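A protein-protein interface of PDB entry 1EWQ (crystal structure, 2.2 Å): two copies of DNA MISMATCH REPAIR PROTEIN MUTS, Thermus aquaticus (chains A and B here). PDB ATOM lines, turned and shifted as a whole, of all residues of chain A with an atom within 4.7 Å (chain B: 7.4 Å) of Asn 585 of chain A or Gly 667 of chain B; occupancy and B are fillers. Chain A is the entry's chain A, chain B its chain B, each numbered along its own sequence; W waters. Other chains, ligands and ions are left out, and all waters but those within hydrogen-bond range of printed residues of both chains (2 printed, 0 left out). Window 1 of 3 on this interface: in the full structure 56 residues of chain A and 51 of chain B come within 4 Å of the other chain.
The backbone NH (N) of Ser 637 of chain B lies close to the side-chain sulfur (SD) of Met 586 of chain A, at 3.6 Å.
The side-chain sulfur of Met 586 of chain A sits close to the side-chain sulfur of Met 640 of chain B (3.6 Å).
NE2 of His 696 of chain A is in hydrogen-bond range of O of Gly 667 of chain B (3.4 Å).
OG of Ser 637 of chain B sits at hydrogen-bond distance from N of Met 640 of chain B.
The side-chain carboxylate of Glu 663 of chain A lies within hydrogen-bond range of a ring nitrogen (NE2) of His 696 of chain A, at 2.7 Å.
The side-chain amide oxygen (OD1) of Asn 585 of chain A sits close to the side-chain carboxylate (OE2) of Glu 663 of chain A, at 3.0 Å.
ND1 of His 696 of chain A sits at hydrogen-bond distance from O of Gly 583 of chain A (3.3 Å).
ND2 of Asn 585 of chain A lies within hydrogen-bond range of NE2 of His 696 of chain A, 2.9 Å away.
Among the printed residues, merely in contact across the chains: Asn 585 of chain A with Ser 637 of chain B, Asn 585 of chain A with Gly 667 of chain B, Met 586 of chain A with Gly 635 of chain B, His 696 of chain A with Thr 668 of chain B and His 696 of chain A with Ser 669 of chain B.
Printed residues of chain B within 4 Å of Asn 585 of chain A: Ser 637 and Gly 667.
Printed residues of chain A within 4 Å of Ser 637 of chain B: Asn 585 (3.7 Å) and Met 586 (3.6 Å).
Glu 642 of chain B touches none of the printed residues of chain A.
Arg 666 of chain B touches none of the printed residues of chain A.
Of chain A, only Asn 585 and His 696 come within 4 Å of Gly 667 of chain B.
Of the printed residues of chain A, Thr 668 of chain B touches His 696 (3.5 Å).
The nearest printed residue of chain A that does not touch Gly 667 of chain B is Glu 663 of chain A (4.9 Å).
The nearest printed residue of chain B that does not touch Met 586 of chain A is Lys 636 of chain B (4.03 Å).
Of the 8 printed residues of chain A, 3 touch a printed residue of chain B.
Printed residues of chain A that touch a printed residue of chain B: Asn 585, Met 586 and His 696.
Hydrophobic or aromatic side chains of chain A that line the printed part of chain B: Met 586 and His 696.
Along chain A the printed residues that touch a printed residue of chain B span positions 585 to 696.
Of the 16 printed residues of chain B, 6 touch a printed residue of chain A.
Printed residues of chain B that touch a printed residue of chain A: Gly 635, Ser 637, Met 640, Gly 667, Thr 668 and Ser 669.
Among the printed residues, 8 pairs touch across the chains.
Position printed for both chains: 663.
Of the 8 pairs that touch across the chains among the printed residues, none has its exchanged pair printed and touching as well.
Water W2 lies within hydrogen-bond range of the side-chain amide nitrogen of Asn 585 of chain A (2.8 Å) and the backbone carbonyl oxygen of Gly 667 of chain B (3.1 Å).
Water W1 lies within hydrogen-bond range of ND2 of Asn 585 of chain A, O of Gly 667 of chain B and N of Phe 639 of chain B.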
ATOM      1  N   GLY A 583      10.801 -26.733   8.513  1.00  0.00           N
ATOM      2  CA  GLY A 583      10.755 -26.137   9.833  1.00  0.00           C
ATOM      3  C   GLY A 583       9.420 -25.442  10.038  1.00  0.00           C
ATOM      4  O   GLY A 583       8.679 -25.232   9.077  1.00  0.00           O
ATOM      5  N   PRO A 584       9.091 -25.055  11.277  1.00  0.00           N
ATOM      6  CA  PRO A 584       7.828 -24.386  11.586  1.00  0.00           C
ATOM      7  C   PRO A 584       7.757 -22.954  11.116  1.00  0.00           C
ATOM      8  O   PRO A 584       8.768 -22.339  10.788  1.00  0.00           O
ATOM      9  CB  PRO A 584       7.773 -24.465  13.100  1.00  0.00           C
ATOM     10  CG  PRO A 584       9.208 -24.253  13.459  1.00  0.00           C
ATOM     11  CD  PRO A 584       9.928 -25.166  12.485  1.00  0.00           C
ATOM     12  N   ASN A 585       6.542 -22.430  11.086  1.00  0.00           N
ATOM     13  CA  ASN A 585       6.318 -21.046  10.719  1.00  0.00           C
ATOM     14  C   ASN A 585       6.681 -20.218  11.961  1.00  0.00           C
ATOM     15  O   ASN A 585       6.927 -20.775  13.032  1.00  0.00           O
ATOM     16  CB  ASN A 585       4.848 -20.844  10.347  1.00  0.00           C
ATOM     17  CG  ASN A 585       4.459 -21.607   9.099  1.00  0.00           C
ATOM     18  OD1 ASN A 585       4.913 -21.285   7.997  1.00  0.00           O
ATOM     19  ND2 ASN A 585       3.616 -22.621   9.261  1.00  0.00           N
ATOM     20  N   MET A 586       6.720 -18.899  11.818  1.00  0.00           N
ATOM     21  CA  MET A 586       7.068 -18.015  12.929  1.00  0.00           C
ATOM     22  C   MET A 586       8.560 -18.081  13.260  1.00  0.00           C
ATOM     23  O   MET A 586       8.993 -17.579  14.291  1.00  0.00           O
ATOM     24  CB  MET A 586       6.250 -18.362  14.182  1.00  0.00           C
ATOM     25  CG  MET A 586       4.746 -18.166  14.027  1.00  0.00           C
ATOM     26  SD  MET A 586       3.771 -18.579  15.659  1.00  0.00           S
ATOM     27  CE  MET A 586       3.906 -20.490  15.569  1.00  0.00           C
ATOM     28  N   ALA A 587       9.341 -18.709  12.391  1.00  0.00           N
ATOM     29  CA  ALA A 587      10.780 -18.809  12.599  1.00  0.00           C
ATOM     30  C   ALA A 587      11.531 -18.074  11.491  1.00  0.00           C
ATOM     31  O   ALA A 587      12.698 -18.358  11.233  1.00  0.00           O
ATOM     32  CB  ALA A 587      11.207 -20.269  12.641  1.00  0.00           C
ATOM     33  N   GLU A 663       5.269 -22.736   0.675  1.00  0.00           N
ATOM     34  CA  GLU A 663       4.290 -23.787   0.944  1.00  0.00           C
ATOM     35  C   GLU A 663       3.375 -24.174  -0.230  1.00  0.00           C
ATOM     36  O   GLU A 663       2.167 -24.384  -0.064  1.00  0.00           O
ATOM     37  CB  GLU A 663       3.455 -23.403   2.177  1.00  0.00           C
ATOM     38  CG  GLU A 663       4.306 -22.901   3.358  1.00  0.00           C
ATOM     39  CD  GLU A 663       3.512 -22.690   4.644  1.00  0.00           C
ATOM     40  OE1 GLU A 663       2.389 -22.157   4.578  1.00  0.00           O
ATOM     41  OE2 GLU A 663       4.018 -23.045   5.728  1.00  0.00           O
ATOM     42  N   HIS A 696       6.534 -27.599   4.578  1.00  0.00           N
ATOM     43  CA  HIS A 696       6.460 -28.430   5.776  1.00  0.00           C
ATOM     44  C   HIS A 696       6.612 -29.884   5.363  1.00  0.00           C
ATOM     45  O   HIS A 696       6.807 -30.754   6.203  1.00  0.00           O
ATOM     46  CB  HIS A 696       5.112 -28.268   6.477  1.00  0.00           C
ATOM     47  CG  HIS A 696       4.918 -26.922   7.091  1.00  0.00           C
ATOM     48  ND1 HIS A 696       5.759 -26.424   8.062  1.00  0.00           N
ATOM     49  CD2 HIS A 696       4.006 -25.951   6.844  1.00  0.00           C
ATOM     50  CE1 HIS A 696       5.377 -25.201   8.384  1.00  0.00           C
ATOM     51  NE2 HIS A 696       4.317 -24.890   7.658  1.00  0.00           N
ATOM     52  N   PHE A 724      10.979 -19.988  19.115  1.00  0.00           N
ATOM     53  CA  PHE A 724      11.366 -20.051  17.707  1.00  0.00           C
ATOM     54  C   PHE A 724      12.695 -19.358  17.407  1.00  0.00           C
ATOM     55  O   PHE A 724      12.882 -18.183  17.724  1.00  0.00           O
ATOM     56  CB  PHE A 724      10.269 -19.451  16.820  1.00  0.00           C
ATOM     57  CG  PHE A 724       8.948 -20.149  16.941  1.00  0.00           C
ATOM     58  CD1 PHE A 724       8.008 -19.727  17.872  1.00  0.00           C
ATOM     59  CD2 PHE A 724       8.668 -21.271  16.167  1.00  0.00           C
ATOM     60  CE1 PHE A 724       6.804 -20.419  18.034  1.00  0.00           C
ATOM     61  CE2 PHE A 724       7.474 -21.967  16.320  1.00  0.00           C
ATOM     62  CZ  PHE A 724       6.540 -21.545  17.254  1.00  0.00           C
ATOM     63  N   GLY B 635       2.350 -11.620  13.683  1.00  0.00           N
ATOM     64  CA  GLY B 635       3.362 -12.519  14.319  1.00  0.00           C
ATOM     65  C   GLY B 635       2.925 -13.974  14.406  1.00  0.00           C
ATOM     66  O   GLY B 635       3.696 -14.874  14.078  1.00  0.00           O
ATOM     67  N   LYS B 636       1.694 -14.211  14.856  1.00  0.00           N
ATOM     68  CA  LYS B 636       1.174 -15.571  14.976  1.00  0.00           C
ATOM     69  C   LYS B 636       0.860 -16.107  13.589  1.00  0.00           C
ATOM     70  O   LYS B 636       0.231 -15.423  12.787  1.00  0.00           O
ATOM     71  CB  LYS B 636      -0.100 -15.585  15.823  1.00  0.00           C
ATOM     72  CG  LYS B 636       0.063 -14.913  17.175  1.00  0.00           C
ATOM     73  CD  LYS B 636      -1.170 -15.103  18.049  1.00  0.00           C
ATOM     74  CE  LYS B 636      -0.830 -14.879  19.521  1.00  0.00           C
ATOM     75  NZ  LYS B 636      -2.032 -15.000  20.391  1.00  0.00           N
ATOM     76  N   SER B 637       1.304 -17.325  13.305  1.00  0.00           N
ATOM     77  CA  SER B 637       1.063 -17.936  12.002  1.00  0.00           C
ATOM     78  C   SER B 637      -0.401 -18.318  11.847  1.00  0.00           C
ATOM     79  O   SER B 637      -1.165 -18.297  12.807  1.00  0.00           O
ATOM     80  CB  SER B 637       1.916 -19.195  11.837  1.00  0.00           C
ATOM     81  OG  SER B 637       1.561 -20.164  12.804  1.00  0.00           O
ATOM     82  N   THR B 638      -0.779 -18.670  10.628  1.00  0.00           N
ATOM     83  CA  THR B 638      -2.138 -19.081  10.343  1.00  0.00           C
ATOM     84  C   THR B 638      -2.493 -20.351  11.126  1.00  0.00           C
ATOM     85  O   THR B 638      -3.609 -20.491  11.623  1.00  0.00           O
ATOM     86  CB  THR B 638      -2.317 -19.340   8.838  1.00  0.00           C
ATOM     87  OG1 THR B 638      -2.141 -18.110   8.129  1.00  0.00           O
ATOM     88  CG2 THR B 638      -3.710 -19.892   8.550  1.00  0.00           C
ATOM     89  N   PHE B 639      -1.537 -21.268  11.231  1.00  0.00           N
ATOM     90  CA  PHE B 639      -1.751 -22.523  11.948  1.00  0.00           C
ATOM     91  C   PHE B 639      -2.015 -22.307  13.438  1.00  0.00           C
ATOM     92  O   PHE B 639      -2.942 -22.897  14.002  1.00  0.00           O
ATOM     93  CB  PHE B 639      -0.536 -23.435  11.775  1.00  0.00           C
ATOM     94  CG  PHE B 639      -0.626 -24.732  12.536  1.00  0.00           C
ATOM     95  CD1 PHE B 639      -1.457 -25.764  12.092  1.00  0.00           C
ATOM     96  CD2 PHE B 639       0.126 -24.924  13.696  1.00  0.00           C
ATOM     97  CE1 PHE B 639      -1.537 -26.978  12.794  1.00  0.00           C
ATOM     98  CE2 PHE B 639       0.055 -26.129  14.409  1.00  0.00           C
ATOM     99  CZ  PHE B 639      -0.778 -27.160  13.957  1.00  0.00           C
ATOM    100  N   MET B 640      -1.214 -21.458  14.077  1.00  0.00           N
ATOM    101  CA  MET B 640      -1.395 -21.222  15.504  1.00  0.00           C
ATOM    102  C   MET B 640      -2.712 -20.519  15.794  1.00  0.00           C
ATOM    103  O   MET B 640      -3.376 -20.823  16.787  1.00  0.00           O
ATOM    104  CB  MET B 640      -0.240 -20.409  16.067  1.00  0.00           C
ATOM    105  CG  MET B 640      -0.268 -20.294  17.580  1.00  0.00           C
ATOM    106  SD  MET B 640       1.248 -19.257  18.163  1.00  0.00           S
ATOM    107  CE  MET B 640       0.408 -17.616  18.452  1.00  0.00           C
ATOM    108  N   GLU B 642      -5.416 -20.810  14.120  1.00  0.00           N
ATOM    109  CA  GLU B 642      -6.439 -21.835  14.004  1.00  0.00           C
ATOM    110  C   GLU B 642      -6.451 -22.781  15.210  1.00  0.00           C
ATOM    111  O   GLU B 642      -7.520 -23.145  15.700  1.00  0.00           O
ATOM    112  CB  GLU B 642      -6.253 -22.594  12.690  1.00  0.00           C
ATOM    113  CG  GLU B 642      -6.727 -21.771  11.494  1.00  0.00           C
ATOM    114  CD  GLU B 642      -6.444 -22.423  10.158  1.00  0.00           C
ATOM    115  OE1 GLU B 642      -6.265 -23.656  10.110  1.00  0.00           O
ATOM    116  OE2 GLU B 642      -6.424 -21.696   9.148  1.00  0.00           O
ATOM    117  N   GLU B 663     -11.345 -27.660   7.458  1.00  0.00           N
ATOM    118  CA  GLU B 663      -9.954 -28.032   7.188  1.00  0.00           C
ATOM    119  C   GLU B 663      -8.995 -27.941   8.383  1.00  0.00           C
ATOM    120  O   GLU B 663      -7.810 -27.670   8.220  1.00  0.00           O
ATOM    121  CB  GLU B 663      -9.410 -27.193   6.027  1.00  0.00           C
ATOM    122  CG  GLU B 663     -10.289 -27.198   4.781  1.00  0.00           C
ATOM    123  CD  GLU B 663      -9.597 -26.580   3.571  1.00  0.00           C
ATOM    124  OE1 GLU B 663      -8.682 -25.748   3.766  1.00  0.00           O
ATOM    125  OE2 GLU B 663      -9.975 -26.915   2.426  1.00  0.00           O
ATOM    126  N   VAL B 664      -9.513 -28.174   9.583  1.00  0.00           N
ATOM    127  CA  VAL B 664      -8.705 -28.136  10.792  1.00  0.00           C
ATOM    128  C   VAL B 664      -7.562 -29.142  10.676  1.00  0.00           C
ATOM    129  O   VAL B 664      -7.786 -30.313  10.360  1.00  0.00           O
ATOM    130  CB  VAL B 664      -9.560 -28.479  12.031  1.00  0.00           C
ATOM    131  CG1 VAL B 664      -8.666 -28.675  13.250  1.00  0.00           C
ATOM    132  CG2 VAL B 664     -10.575 -27.363  12.281  1.00  0.00           C
ATOM    133  N   GLY B 665      -6.333 -28.681  10.913  1.00  0.00           N
ATOM    134  CA  GLY B 665      -5.196 -29.579  10.826  1.00  0.00           C
ATOM    135  C   GLY B 665      -4.191 -29.133   9.783  1.00  0.00           C
ATOM    136  O   GLY B 665      -3.014 -29.497   9.854  1.00  0.00           O
ATOM    137  N   ARG B 666      -4.661 -28.336   8.823  1.00  0.00           N
ATOM    138  CA  ARG B 666      -3.821 -27.802   7.747  1.00  0.00           C
ATOM    139  C   ARG B 666      -2.783 -26.822   8.294  1.00  0.00           C
ATOM    140  O   ARG B 666      -2.896 -26.361   9.423  1.00  0.00           O
ATOM    141  CB  ARG B 666      -4.689 -27.059   6.723  1.00  0.00           C
ATOM    142  CG  ARG B 666      -5.324 -25.783   7.285  1.00  0.00           C
ATOM    143  CD  ARG B 666      -6.259 -25.081   6.275  1.00  0.00           C
ATOM    144  NE  ARG B 666      -6.930 -23.928   6.873  1.00  0.00           N
ATOM    145  CZ  ARG B 666      -7.849 -23.178   6.265  1.00  0.00           C
ATOM    146  NH1 ARG B 666      -8.231 -23.449   5.020  1.00  0.00           N
ATOM    147  NH2 ARG B 666      -8.378 -22.141   6.900  1.00  0.00           N
ATOM    148  N   GLY B 667      -1.781 -26.511   7.472  1.00  0.00           N
ATOM    149  CA  GLY B 667      -0.750 -25.565   7.855  1.00  0.00           C
ATOM    150  C   GLY B 667       0.484 -26.106   8.556  1.00  0.00           C
ATOM    151  O   GLY B 667       1.293 -25.327   9.059  1.00  0.00           O
ATOM    152  N   THR B 668       0.641 -27.423   8.611  1.00  0.00           N
ATOM    153  CA  THR B 668       1.808 -28.000   9.266  1.00  0.00           C
ATOM    154  C   THR B 668       2.293 -29.202   8.464  1.00  0.00           C
ATOM    155  O   THR B 668       1.933 -29.337   7.303  1.00  0.00           O
ATOM    156  CB  THR B 668       1.487 -28.415  10.735  1.00  0.00           C
ATOM    157  OG1 THR B 668       2.688 -28.856  11.376  1.00  0.00           O
ATOM    158  CG2 THR B 668       0.453 -29.530  10.776  1.00  0.00           C
ATOM    159  N   SER B 669       3.117 -30.061   9.059  1.00  0.00           N
ATOM    160  CA  SER B 669       3.612 -31.241   8.341  1.00  0.00           C
ATOM    161  C   SER B 669       2.479 -32.256   8.154  1.00  0.00           C
ATOM    162  O   SER B 669       1.494 -32.249   8.888  1.00  0.00           O
ATOM    163  CB  SER B 669       4.786 -31.879   9.102  1.00  0.00           C
ATOM    164  OG  SER B 669       4.400 -32.276  10.414  1.00  0.00           O
ATOM    165  N   GLY B 673      -0.315 -32.955  10.965  1.00  0.00           N
ATOM    166  CA  GLY B 673      -1.605 -32.453  10.539  1.00  0.00           C
ATOM    167  C   GLY B 673      -2.724 -33.457  10.747  1.00  0.00           C
ATOM    168  O   GLY B 673      -3.769 -33.122  11.304  1.00  0.00           O
ATOM    169  N   TYR B 697      -8.918 -34.767   4.614  1.00  0.00           N
ATOM    170  CA  TYR B 697      -8.323 -35.977   5.181  1.00  0.00           C
ATOM    171  C   TYR B 697      -9.200 -37.208   5.035  1.00  0.00           C
ATOM    172  O   TYR B 697     -10.012 -37.494   5.918  1.00  0.00           O
ATOM    173  CB  TYR B 697      -8.030 -35.779   6.671  1.00  0.00           C
ATOM    174  CG  TYR B 697      -6.908 -34.817   6.980  1.00  0.00           C
ATOM    175  CD1 TYR B 697      -6.883 -34.125   8.188  1.00  0.00           C
ATOM    176  CD2 TYR B 697      -5.854 -34.624   6.090  1.00  0.00           C
ATOM    177  CE1 TYR B 697      -5.838 -33.266   8.507  1.00  0.00           C
ATOM    178  CE2 TYR B 697      -4.799 -33.763   6.398  1.00  0.00           C
ATOM    179  CZ  TYR B 697      -4.799 -33.091   7.614  1.00  0.00           C
ATOM    180  OH  TYR B 697      -3.750 -32.268   7.950  1.00  0.00           O
HETATM  181  O   HOH W   1       0.743 -22.339   8.856  1.00  0.00           O
HETATM  182  O   HOH W   2       2.847 -24.159  11.528  1.00  0.00           O
